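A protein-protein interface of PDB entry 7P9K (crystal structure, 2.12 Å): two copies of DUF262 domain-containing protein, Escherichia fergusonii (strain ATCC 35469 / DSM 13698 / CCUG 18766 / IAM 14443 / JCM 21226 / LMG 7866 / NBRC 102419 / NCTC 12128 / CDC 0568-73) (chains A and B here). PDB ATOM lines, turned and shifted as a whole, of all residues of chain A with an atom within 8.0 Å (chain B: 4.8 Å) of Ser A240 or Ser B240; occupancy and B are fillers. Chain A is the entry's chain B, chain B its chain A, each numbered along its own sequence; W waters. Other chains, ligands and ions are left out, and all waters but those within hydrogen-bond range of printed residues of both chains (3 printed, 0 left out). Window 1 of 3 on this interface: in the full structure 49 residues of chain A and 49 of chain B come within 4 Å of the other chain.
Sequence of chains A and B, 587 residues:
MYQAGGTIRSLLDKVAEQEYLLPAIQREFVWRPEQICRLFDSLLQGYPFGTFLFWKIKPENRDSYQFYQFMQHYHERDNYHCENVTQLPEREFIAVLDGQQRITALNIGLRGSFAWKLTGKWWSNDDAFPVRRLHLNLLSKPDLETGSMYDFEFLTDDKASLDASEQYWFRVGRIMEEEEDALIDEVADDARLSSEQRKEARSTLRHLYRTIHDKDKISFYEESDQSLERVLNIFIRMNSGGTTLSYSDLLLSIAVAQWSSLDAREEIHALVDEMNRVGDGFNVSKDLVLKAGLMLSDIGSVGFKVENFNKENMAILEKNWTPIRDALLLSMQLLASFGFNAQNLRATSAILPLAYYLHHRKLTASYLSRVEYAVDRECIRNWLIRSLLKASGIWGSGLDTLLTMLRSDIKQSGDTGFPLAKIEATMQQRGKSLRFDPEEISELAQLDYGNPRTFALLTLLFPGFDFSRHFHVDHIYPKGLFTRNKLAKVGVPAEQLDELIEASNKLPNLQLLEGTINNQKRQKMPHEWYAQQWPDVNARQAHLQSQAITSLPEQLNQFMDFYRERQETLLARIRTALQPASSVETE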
ATOM      1  N   PHE A  49       7.216   6.754  -2.967  1.00  0.00           N
ATOM      2  CA  PHE A  49       6.281   7.800  -2.549  1.00  0.00           C
ATOM      3  C   PHE A  49       4.851   7.402  -2.891  1.00  0.00           C
ATOM      4  O   PHE A  49       4.596   6.804  -3.940  1.00  0.00           O
ATOM      5  CB  PHE A  49       6.586   9.109  -3.270  1.00  0.00           C
ATOM      6  CG  PHE A  49       7.564   9.983  -2.575  1.00  0.00           C
ATOM      7  CD1 PHE A  49       7.369  10.357  -1.256  1.00  0.00           C
ATOM      8  CD2 PHE A  49       8.672  10.455  -3.248  1.00  0.00           C
ATOM      9  CE1 PHE A  49       8.274  11.190  -0.623  1.00  0.00           C
ATOM     10  CE2 PHE A  49       9.582  11.280  -2.619  1.00  0.00           C
ATOM     11  CZ  PHE A  49       9.390  11.645  -1.307  1.00  0.00           C
ATOM     12  N   GLY A  50       3.906   7.752  -2.018  1.00  0.00           N
ATOM     13  CA  GLY A  50       2.512   7.667  -2.395  1.00  0.00           C
ATOM     14  C   GLY A  50       2.153   8.755  -3.387  1.00  0.00           C
ATOM     15  O   GLY A  50       2.878   9.733  -3.564  1.00  0.00           O
ATOM     16  N   THR A  51       1.012   8.589  -4.054  1.00  0.00           N
ATOM     17  CA  THR A  51       0.593   9.559  -5.061  1.00  0.00           C
ATOM     18  C   THR A  51       0.202  10.896  -4.415  1.00  0.00           C
ATOM     19  O   THR A  51      -0.329  10.940  -3.301  1.00  0.00           O
ATOM     20  CB  THR A  51      -0.570   8.982  -5.878  1.00  0.00           C
ATOM     21  OG1 THR A  51      -0.143   7.765  -6.508  1.00  0.00           O
ATOM     22  CG2 THR A  51      -1.032   9.957  -6.968  1.00  0.00           C
ATOM     23  N   PHE A  52       0.500  11.992  -5.108  1.00  0.00           N
ATOM     24  CA  PHE A  52       0.102  13.326  -4.686  1.00  0.00           C
ATOM     25  C   PHE A  52      -1.189  13.717  -5.393  1.00  0.00           C
ATOM     26  O   PHE A  52      -1.624  13.070  -6.346  1.00  0.00           O
ATOM     27  CB  PHE A  52       1.170  14.380  -5.013  1.00  0.00           C
ATOM     28  CG  PHE A  52       2.529  14.105  -4.440  1.00  0.00           C
ATOM     29  CD1 PHE A  52       2.690  13.309  -3.329  1.00  0.00           C
ATOM     30  CD2 PHE A  52       3.663  14.662  -5.036  1.00  0.00           C
ATOM     31  CE1 PHE A  52       3.961  13.061  -2.817  1.00  0.00           C
ATOM     32  CE2 PHE A  52       4.938  14.426  -4.518  1.00  0.00           C
ATOM     33  CZ  PHE A  52       5.082  13.619  -3.412  1.00  0.00           C
ATOM     34  N   LEU A  53      -1.768  14.827  -4.961  1.00  0.00           N
ATOM     35  CA  LEU A  53      -2.970  15.378  -5.583  1.00  0.00           C
ATOM     36  C   LEU A  53      -2.768  16.869  -5.816  1.00  0.00           C
ATOM     37  O   LEU A  53      -2.467  17.616  -4.875  1.00  0.00           O
ATOM     38  CB  LEU A  53      -4.229  15.132  -4.710  1.00  0.00           C
ATOM     39  CG  LEU A  53      -5.560  15.762  -5.164  1.00  0.00           C
ATOM     40  CD1 LEU A  53      -6.125  15.053  -6.389  1.00  0.00           C
ATOM     41  CD2 LEU A  53      -6.576  15.751  -4.053  1.00  0.00           C
ATOM     42  N   ASP A  98      -2.405  17.385  -1.760  1.00  0.00           N
ATOM     43  CA  ASP A  98      -1.813  16.275  -1.027  1.00  0.00           C
ATOM     44  C   ASP A  98      -0.374  16.093  -1.512  1.00  0.00           C
ATOM     45  O   ASP A  98      -0.118  16.018  -2.719  1.00  0.00           O
ATOM     46  CB  ASP A  98      -2.628  14.993  -1.226  1.00  0.00           C
ATOM     47  CG  ASP A  98      -2.436  13.991  -0.090  1.00  0.00           C
ATOM     48  OD1 ASP A  98      -3.032  14.186   1.003  1.00  0.00           O
ATOM     49  OD2 ASP A  98      -1.684  13.004  -0.300  1.00  0.00           O
ATOM     50  N   GLY A  99       0.564  16.067  -0.573  1.00  0.00           N
ATOM     51  CA  GLY A  99       1.980  16.032  -0.891  1.00  0.00           C
ATOM     52  C   GLY A  99       2.760  17.179  -0.289  1.00  0.00           C
ATOM     53  O   GLY A  99       3.987  17.236  -0.463  1.00  0.00           O
ATOM     54  N   ARG A 102       5.828  16.177   2.126  1.00  0.00           N
ATOM     55  CA  ARG A 102       6.870  15.447   1.422  1.00  0.00           C
ATOM     56  C   ARG A 102       7.603  16.362   0.468  1.00  0.00           C
ATOM     57  O   ARG A 102       8.835  16.290   0.348  1.00  0.00           O
ATOM     58  CB  ARG A 102       6.269  14.259   0.679  1.00  0.00           C
ATOM     59  CG  ARG A 102       5.863  13.140   1.635  1.00  0.00           C
ATOM     60  CD  ARG A 102       4.917  12.182   0.966  1.00  0.00           C
ATOM     61  NE  ARG A 102       3.576  12.732   0.852  1.00  0.00           N
ATOM     62  CZ  ARG A 102       2.545  12.069   0.342  1.00  0.00           C
ATOM     63  NH1 ARG A 102       2.723  10.837  -0.115  1.00  0.00           N
ATOM     64  NH2 ARG A 102       1.337  12.635   0.295  1.00  0.00           N
ATOM     65  N   PHE A 235      -9.430   9.960  -4.985  1.00  0.00           N
ATOM     66  CA  PHE A 235      -8.075   9.900  -4.444  1.00  0.00           C
ATOM     67  C   PHE A 235      -8.068   9.473  -2.981  1.00  0.00           C
ATOM     68  O   PHE A 235      -7.216   8.680  -2.558  1.00  0.00           O
ATOM     69  CB  PHE A 235      -7.394  11.256  -4.612  1.00  0.00           C
ATOM     70  CG  PHE A 235      -6.062  11.351  -3.946  1.00  0.00           C
ATOM     71  CD1 PHE A 235      -4.903  10.959  -4.609  1.00  0.00           C
ATOM     72  CD2 PHE A 235      -5.962  11.820  -2.647  1.00  0.00           C
ATOM     73  CE1 PHE A 235      -3.680  11.072  -3.991  1.00  0.00           C
ATOM     74  CE2 PHE A 235      -4.736  11.921  -2.012  1.00  0.00           C
ATOM     75  CZ  PHE A 235      -3.594  11.550  -2.682  1.00  0.00           C
ATOM     76  N   ILE A 236      -9.004   9.989  -2.193  1.00  0.00           N
ATOM     77  CA  ILE A 236      -9.078   9.605  -0.786  1.00  0.00           C
ATOM     78  C   ILE A 236      -9.545   8.157  -0.638  1.00  0.00           C
ATOM     79  O   ILE A 236      -9.054   7.421   0.221  1.00  0.00           O
ATOM     80  CB  ILE A 236     -10.000  10.576  -0.026  1.00  0.00           C
ATOM     81  CG1 ILE A 236      -9.332  11.946   0.090  1.00  0.00           C
ATOM     82  CG2 ILE A 236     -10.353  10.036   1.360  1.00  0.00           C
ATOM     83  CD1 ILE A 236     -10.194  12.966   0.804  1.00  0.00           C
ATOM     84  N   ARG A 237     -10.516   7.738  -1.456  1.00  0.00           N
ATOM     85  CA  ARG A 237     -10.997   6.355  -1.435  1.00  0.00           C
ATOM     86  C   ARG A 237      -9.870   5.349  -1.675  1.00  0.00           C
ATOM     87  O   ARG A 237      -9.741   4.372  -0.937  1.00  0.00           O
ATOM     88  CB  ARG A 237     -12.092   6.166  -2.494  1.00  0.00           C
ATOM     89  CG  ARG A 237     -13.509   6.265  -1.985  1.00  0.00           C
ATOM     90  CD  ARG A 237     -13.715   7.571  -1.219  1.00  0.00           C
ATOM     91  NE  ARG A 237     -14.557   7.358  -0.046  1.00  0.00           N
ATOM     92  CZ  ARG A 237     -14.862   8.304   0.834  1.00  0.00           C
ATOM     93  NH1 ARG A 237     -15.637   8.009   1.880  1.00  0.00           N
ATOM     94  NH2 ARG A 237     -14.398   9.540   0.660  1.00  0.00           N
ATOM     95  N   MET A 238      -9.054   5.560  -2.717  1.00  0.00           N
ATOM     96  CA  MET A 238      -8.088   4.553  -3.161  1.00  0.00           C
ATOM     97  C   MET A 238      -6.731   4.621  -2.456  1.00  0.00           C
ATOM     98  O   MET A 238      -5.982   3.639  -2.488  1.00  0.00           O
ATOM     99  CB  MET A 238      -7.859   4.663  -4.682  1.00  0.00           C
ATOM    100  CG  MET A 238      -9.140   4.780  -5.515  1.00  0.00           C
ATOM    101  SD  MET A 238     -10.209   3.336  -5.376  1.00  0.00           S
ATOM    102  CE  MET A 238      -9.331   2.149  -6.394  1.00  0.00           C
ATOM    103  N   ASN A 239      -6.367   5.746  -1.848  1.00  0.00           N
ATOM    104  CA  ASN A 239      -5.099   5.839  -1.130  1.00  0.00           C
ATOM    105  C   ASN A 239      -5.379   5.846   0.378  1.00  0.00           C
ATOM    106  O   ASN A 239      -6.480   5.490   0.811  1.00  0.00           O
ATOM    107  CB  ASN A 239      -4.339   7.064  -1.628  1.00  0.00           C
ATOM    108  CG  ASN A 239      -4.041   6.990  -3.120  1.00  0.00           C
ATOM    109  OD1 ASN A 239      -3.070   6.356  -3.547  1.00  0.00           O
ATOM    110  ND2 ASN A 239      -4.885   7.621  -3.921  1.00  0.00           N
ATOM    111  N   SER A 240      -4.396   6.241   1.187  1.00  0.00           N
ATOM    112  CA  SER A 240      -4.693   6.407   2.614  1.00  0.00           C
ATOM    113  C   SER A 240      -5.719   7.519   2.835  1.00  0.00           C
ATOM    114  O   SER A 240      -5.352   8.697   2.960  1.00  0.00           O
ATOM    115  CB  SER A 240      -3.420   6.705   3.423  1.00  0.00           C
ATOM    116  OG  SER A 240      -2.606   5.560   3.566  1.00  0.00           O
ATOM    117  N   GLY A 241      -7.001   7.160   2.903  1.00  0.00           N
ATOM    118  CA  GLY A 241      -8.042   8.163   3.046  1.00  0.00           C
ATOM    119  C   GLY A 241      -8.334   8.523   4.491  1.00  0.00           C
ATOM    120  O   GLY A 241      -8.036   9.638   4.950  1.00  0.00           O
ATOM    121  N   GLY A 242      -8.947   7.579   5.209  1.00  0.00           N
ATOM    122  CA  GLY A 242      -9.040   7.652   6.652  1.00  0.00           C
ATOM    123  C   GLY A 242      -7.653   7.527   7.245  1.00  0.00           C
ATOM    124  O   GLY A 242      -7.081   6.431   7.281  1.00  0.00           O
ATOM    125  N   THR A 243      -7.107   8.661   7.690  1.00  0.00           N
ATOM    126  CA  THR A 243      -5.710   8.769   8.094  1.00  0.00           C
ATOM    127  C   THR A 243      -5.254   7.548   8.892  1.00  0.00           C
ATOM    128  O   THR A 243      -6.019   6.967   9.673  1.00  0.00           O
ATOM    129  CB  THR A 243      -5.520  10.057   8.913  1.00  0.00           C
ATOM    130  OG1 THR A 243      -4.260  10.040   9.600  1.00  0.00           O
ATOM    131  CG2 THR A 243      -6.654  10.232   9.921  1.00  0.00           C
ATOM    132  N   THR A 244      -4.000   7.155   8.659  1.00  0.00           N
ATOM    133  CA  THR A 244      -3.361   6.074   9.403  1.00  0.00           C
ATOM    134  C   THR A 244      -3.113   6.489  10.851  1.00  0.00           C
ATOM    135  O   THR A 244      -2.821   7.649  11.147  1.00  0.00           O
ATOM    136  CB  THR A 244      -2.023   5.693   8.751  1.00  0.00           C
ATOM    137  OG1 THR A 244      -2.157   5.719   7.326  1.00  0.00           O
ATOM    138  CG2 THR A 244      -1.559   4.302   9.198  1.00  0.00           C
ATOM    139  N   ASP B  98      -3.492  -0.418   7.880  1.00  0.00           N
ATOM    140  CA  ASP B  98      -3.871   0.563   6.868  1.00  0.00           C
ATOM    141  C   ASP B  98      -4.420  -0.190   5.666  1.00  0.00           C
ATOM    142  O   ASP B  98      -3.788  -1.134   5.188  1.00  0.00           O
ATOM    143  CB  ASP B  98      -2.681   1.430   6.455  1.00  0.00           C
ATOM    144  CG  ASP B  98      -3.113   2.721   5.787  1.00  0.00           C
ATOM    145  OD1 ASP B  98      -3.655   3.608   6.495  1.00  0.00           O
ATOM    146  OD2 ASP B  98      -2.918   2.844   4.550  1.00  0.00           O
ATOM    147  N   ARG B 102     -10.813  -0.027   2.681  1.00  0.00           N
ATOM    148  CA  ARG B 102     -10.776  -0.467   1.291  1.00  0.00           C
ATOM    149  C   ARG B 102     -10.979  -1.970   1.196  1.00  0.00           C
ATOM    150  O   ARG B 102     -11.672  -2.449   0.285  1.00  0.00           O
ATOM    151  CB  ARG B 102      -9.460  -0.049   0.633  1.00  0.00           C
ATOM    152  CG  ARG B 102      -9.440   1.405   0.175  1.00  0.00           C
ATOM    153  CD  ARG B 102      -8.033   1.904  -0.015  1.00  0.00           C
ATOM    154  NE  ARG B 102      -7.338   2.083   1.255  1.00  0.00           N
ATOM    155  CZ  ARG B 102      -6.026   2.273   1.368  1.00  0.00           C
ATOM    156  NH1 ARG B 102      -5.272   2.322   0.277  1.00  0.00           N
ATOM    157  NH2 ARG B 102      -5.469   2.423   2.567  1.00  0.00           N
ATOM    158  N   PHE B 235       6.183   4.347   6.428  1.00  0.00           N
ATOM    159  CA  PHE B 235       4.923   4.282   5.693  1.00  0.00           C
ATOM    160  C   PHE B 235       4.188   5.614   5.736  1.00  0.00           C
ATOM    161  O   PHE B 235       3.760   6.128   4.703  1.00  0.00           O
ATOM    162  CB  PHE B 235       4.044   3.182   6.263  1.00  0.00           C
ATOM    163  CG  PHE B 235       2.722   3.044   5.566  1.00  0.00           C
ATOM    164  CD1 PHE B 235       2.608   2.273   4.410  1.00  0.00           C
ATOM    165  CD2 PHE B 235       1.589   3.662   6.074  1.00  0.00           C
ATOM    166  CE1 PHE B 235       1.390   2.134   3.774  1.00  0.00           C
ATOM    167  CE2 PHE B 235       0.361   3.535   5.436  1.00  0.00           C
ATOM    168  CZ  PHE B 235       0.258   2.763   4.296  1.00  0.00           C
ATOM    169  N   ILE B 236       4.050   6.197   6.927  1.00  0.00           N
ATOM    170  CA  ILE B 236       3.299   7.439   7.075  1.00  0.00           C
ATOM    171  C   ILE B 236       4.019   8.605   6.401  1.00  0.00           C
ATOM    172  O   ILE B 236       3.384   9.433   5.739  1.00  0.00           O
ATOM    173  CB  ILE B 236       3.024   7.719   8.568  1.00  0.00           C
ATOM    174  CG1 ILE B 236       1.944   6.772   9.097  1.00  0.00           C
ATOM    175  CG2 ILE B 236       2.521   9.115   8.771  1.00  0.00           C
ATOM    176  CD1 ILE B 236       1.809   6.785  10.623  1.00  0.00           C
ATOM    177  N   MET B 238       6.085   8.506   3.800  1.00  0.00           N
ATOM    178  CA  MET B 238       6.116   8.354   2.344  1.00  0.00           C
ATOM    179  C   MET B 238       4.731   8.409   1.697  1.00  0.00           C
ATOM    180  O   MET B 238       4.637   8.715   0.502  1.00  0.00           O
ATOM    181  CB  MET B 238       6.804   7.032   1.944  1.00  0.00           C
ATOM    182  CG  MET B 238       8.250   6.837   2.438  1.00  0.00           C
ATOM    183  SD  MET B 238       9.328   8.271   2.238  1.00  0.00           S
ATOM    184  CE  MET B 238       9.884   7.991   0.538  1.00  0.00           C
ATOM    185  N   ASN B 239       3.654   8.119   2.429  1.00  0.00           N
ATOM    186  CA  ASN B 239       2.319   8.180   1.844  1.00  0.00           C
ATOM    187  C   ASN B 239       1.572   9.393   2.384  1.00  0.00           C
ATOM    188  O   ASN B 239       2.160  10.277   3.022  1.00  0.00           O
ATOM    189  CB  ASN B 239       1.571   6.877   2.100  1.00  0.00           C
ATOM    190  CG  ASN B 239       2.213   5.706   1.394  1.00  0.00           C
ATOM    191  OD1 ASN B 239       1.744   5.258   0.346  1.00  0.00           O
ATOM    192  ND2 ASN B 239       3.313   5.220   1.948  1.00  0.00           N
ATOM    193  N   SER B 240       0.268   9.464   2.098  1.00  0.00           N
ATOM    194  CA  SER B 240      -0.537  10.519   2.710  1.00  0.00           C
ATOM    195  C   SER B 240      -0.289  10.452   4.204  1.00  0.00           C
ATOM    196  O   SER B 240      -0.786   9.544   4.882  1.00  0.00           O
ATOM    197  CB  SER B 240      -2.035  10.379   2.380  1.00  0.00           C
ATOM    198  OG  SER B 240      -2.255   9.993   1.026  1.00  0.00           O
ATOM    199  N   GLY B 241       0.514  11.373   4.717  1.00  0.00           N
ATOM    200  CA  GLY B 241       0.946  11.297   6.096  1.00  0.00           C
ATOM    201  C   GLY B 241       0.036  12.107   6.984  1.00  0.00           C
ATOM    202  O   GLY B 241      -0.314  11.687   8.093  1.00  0.00           O
ATOM    203  N   GLY B 242      -0.344  13.284   6.495  1.00  0.00           N
ATOM    204  CA  GLY B 242      -1.392  14.068   7.128  1.00  0.00           C
ATOM    205  C   GLY B 242      -2.741  13.723   6.518  1.00  0.00           C
ATOM    206  O   GLY B 242      -2.878  13.625   5.299  1.00  0.00           O
ATOM    207  N   THR B 244      -5.622  13.473   4.578  1.00  0.00           N
ATOM    208  CA  THR B 244      -6.024  14.231   3.406  1.00  0.00           C
ATOM    209  C   THR B 244      -7.337  14.945   3.686  1.00  0.00           C
ATOM    210  O   THR B 244      -8.298  14.331   4.156  1.00  0.00           O
ATOM    211  CB  THR B 244      -6.168  13.298   2.201  1.00  0.00           C
ATOM    212  OG1 THR B 244      -5.122  12.307   2.217  1.00  0.00           O
ATOM    213  CG2 THR B 244      -6.123  14.110   0.900  1.00  0.00           C
HETATM  214  O   HOH W   1      -0.151   9.610  -0.800  1.00  0.00           O
HETATM  215  O   HOH W   2      -2.133  14.909   3.288  1.00  0.00           O
HETATM  216  O   HOH W   3      -2.549   3.800   1.052  1.00  0.00           O
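The side-chain hydroxyl (OG) of Ser A240 lies within hydrogen-bond range of the side-chain carboxylate (OD2) of Asp B98, 2.9 Å away.
The side-chain carboxylate of Asp B98 sits at hydrogen-bond distance from the side-chain hydroxyl of Thr A244 (2.7 Å).
NH1 of Arg B102 is in hydrogen-bond range of O of Met A238 (3.1 Å).
NH1 of Arg B102 lies close to O of Asn A239, at 3.4 Å.
O of Met B238 is in hydrogen-bond range of N of Gly A50, 2.8 Å away.
NH1 of Arg A102 sits at hydrogen-bond distance from O of Met B238, 2.9 Å away.
O of Asn B239 sits close to NH1 of Arg A102 (3.2 Å).
OD2 of Asp A98 lies within hydrogen-bond range of OG of Ser B240, at 3.3 Å.
The side-chain hydroxyl of Thr B244 lies within hydrogen-bond range of the side-chain carboxylate of Asp A98.
The guanidinium group (NH2) of Arg B102 is in salt-bridge range of the side-chain carboxylate (OD2) of Asp B98 (3.3 Å).
The side-chain amide nitrogen of Asn B239 lies within hydrogen-bond range of the backbone carbonyl oxygen of Phe B235.
N of Leu A53 lies within hydrogen-bond range of O of Asp A98 (3.0 Å).
OD2 of Asp A98 is in salt-bridge range of NH2 of Arg A102 (3.1 Å).
The backbone carbonyl oxygen of Phe A235 lies within hydrogen-bond range of the side-chain amide nitrogen of Asn A239.
The backbone carbonyl oxygen of Ile A236 sits close to the backbone NH of Gly A241.
Among the printed residues, merely in contact across the chains: Arg A237 with Arg B102 (3.1 Å), Arg A102 with Ser B240 (3.6 Å), Phe A49 with Met B238 (3.6 Å), Ser A240 with Thr B244 (3.7 Å), Gly A50 with Asn B239 (3.7 Å), Ser A240 with Ser B240 (3.8 Å), Thr A244 with Phe B235 (3.8 Å), Phe A235 with Thr B244 (3.9 Å) and Ile A236 with Thr B244 (3.95 Å).
Of the printed residues of chain B, Gly A50 touches Met B238 and Asn B239.
Phe A52 touches none of the printed residues of chain B.
Of the printed residues of chain B, Arg A102 touches Met B238 (2.9 Å), Asn B239 (3.1 Å) and Ser B240 (3.6 Å).
Printed residues of chain A within 4 Å of Asp B98: Ser A240 (2.9 Å) and Thr A244 (2.7 Å).
Of the printed residues of chain A, Phe B235 touches Thr A244.
Of the printed residues of chain A, Asn B239 touches Gly A50 (3.7 Å) and Arg A102 (3.1 Å).
Of chain A, only Asp A98, Arg A102 and Ser A240 come within 4 Å of Ser B240.
Gly B242 touches none of the printed residues of chain A.
The nearest printed residue of chain B that does not touch Ser A240 is Phe B235 (4.05 Å).
The nearest residue of chain A that does not touch Ser B240 is Phe A235 (4.2 Å).
The nearest printed residue of chain B that does not touch Met A238 is Asp B98 (7.7 Å).
Of the 18 printed residues of chain A, 11 touch a printed residue of chain B.
Hydrophobic or aromatic side chains of chain A that line the printed part of chain B: Phe A49, Phe A235 and Ile A236.
Of the 10 printed residues of chain B, 7 touch a printed residue of chain A.
Hydrophobic or aromatic side chains of chain B within 4 Å of the printed part of chain A: Phe B235 and Met B238.
Among the printed residues, no Asp or Glu carboxylate lies within 4 Å of a Lys or Arg side-chain nitrogen of the other chain.
Asp A98 touches Thr B244, and with the chains exchanged Thr A244 touches Asp B98.
Arg A102 touches Met B238, and with the chains exchanged Met A238 touches Arg B102.
Arg A102 touches Asn B239, and with the chains exchanged Asn A239 touches Arg B102.
Phe A235 touches Thr B244, and with the chains exchanged Thr A244 touches Phe B235.
Positions printed for both chains: 98, 102, 235, 236, 238, 239, 240, 241, 242 and 244.
Water W2 lies within hydrogen-bond range of O of Gly B242 (2.5 Å) and OD1 of Asp A98 (2.6 Å).
Water W1 lies within hydrogen-bond range of the side-chain hydroxyl (OG) of Ser B240 (2.8 Å), the backbone carbonyl oxygen (O) of Thr A51 (2.8 Å) and the guanidinium group (NH1) of Arg A102 (3.2 Å).
Water W3 lies within hydrogen-bond range of N of Ser A240 (3.1 Å) and NH1 of Arg B102 (3.2 Å).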
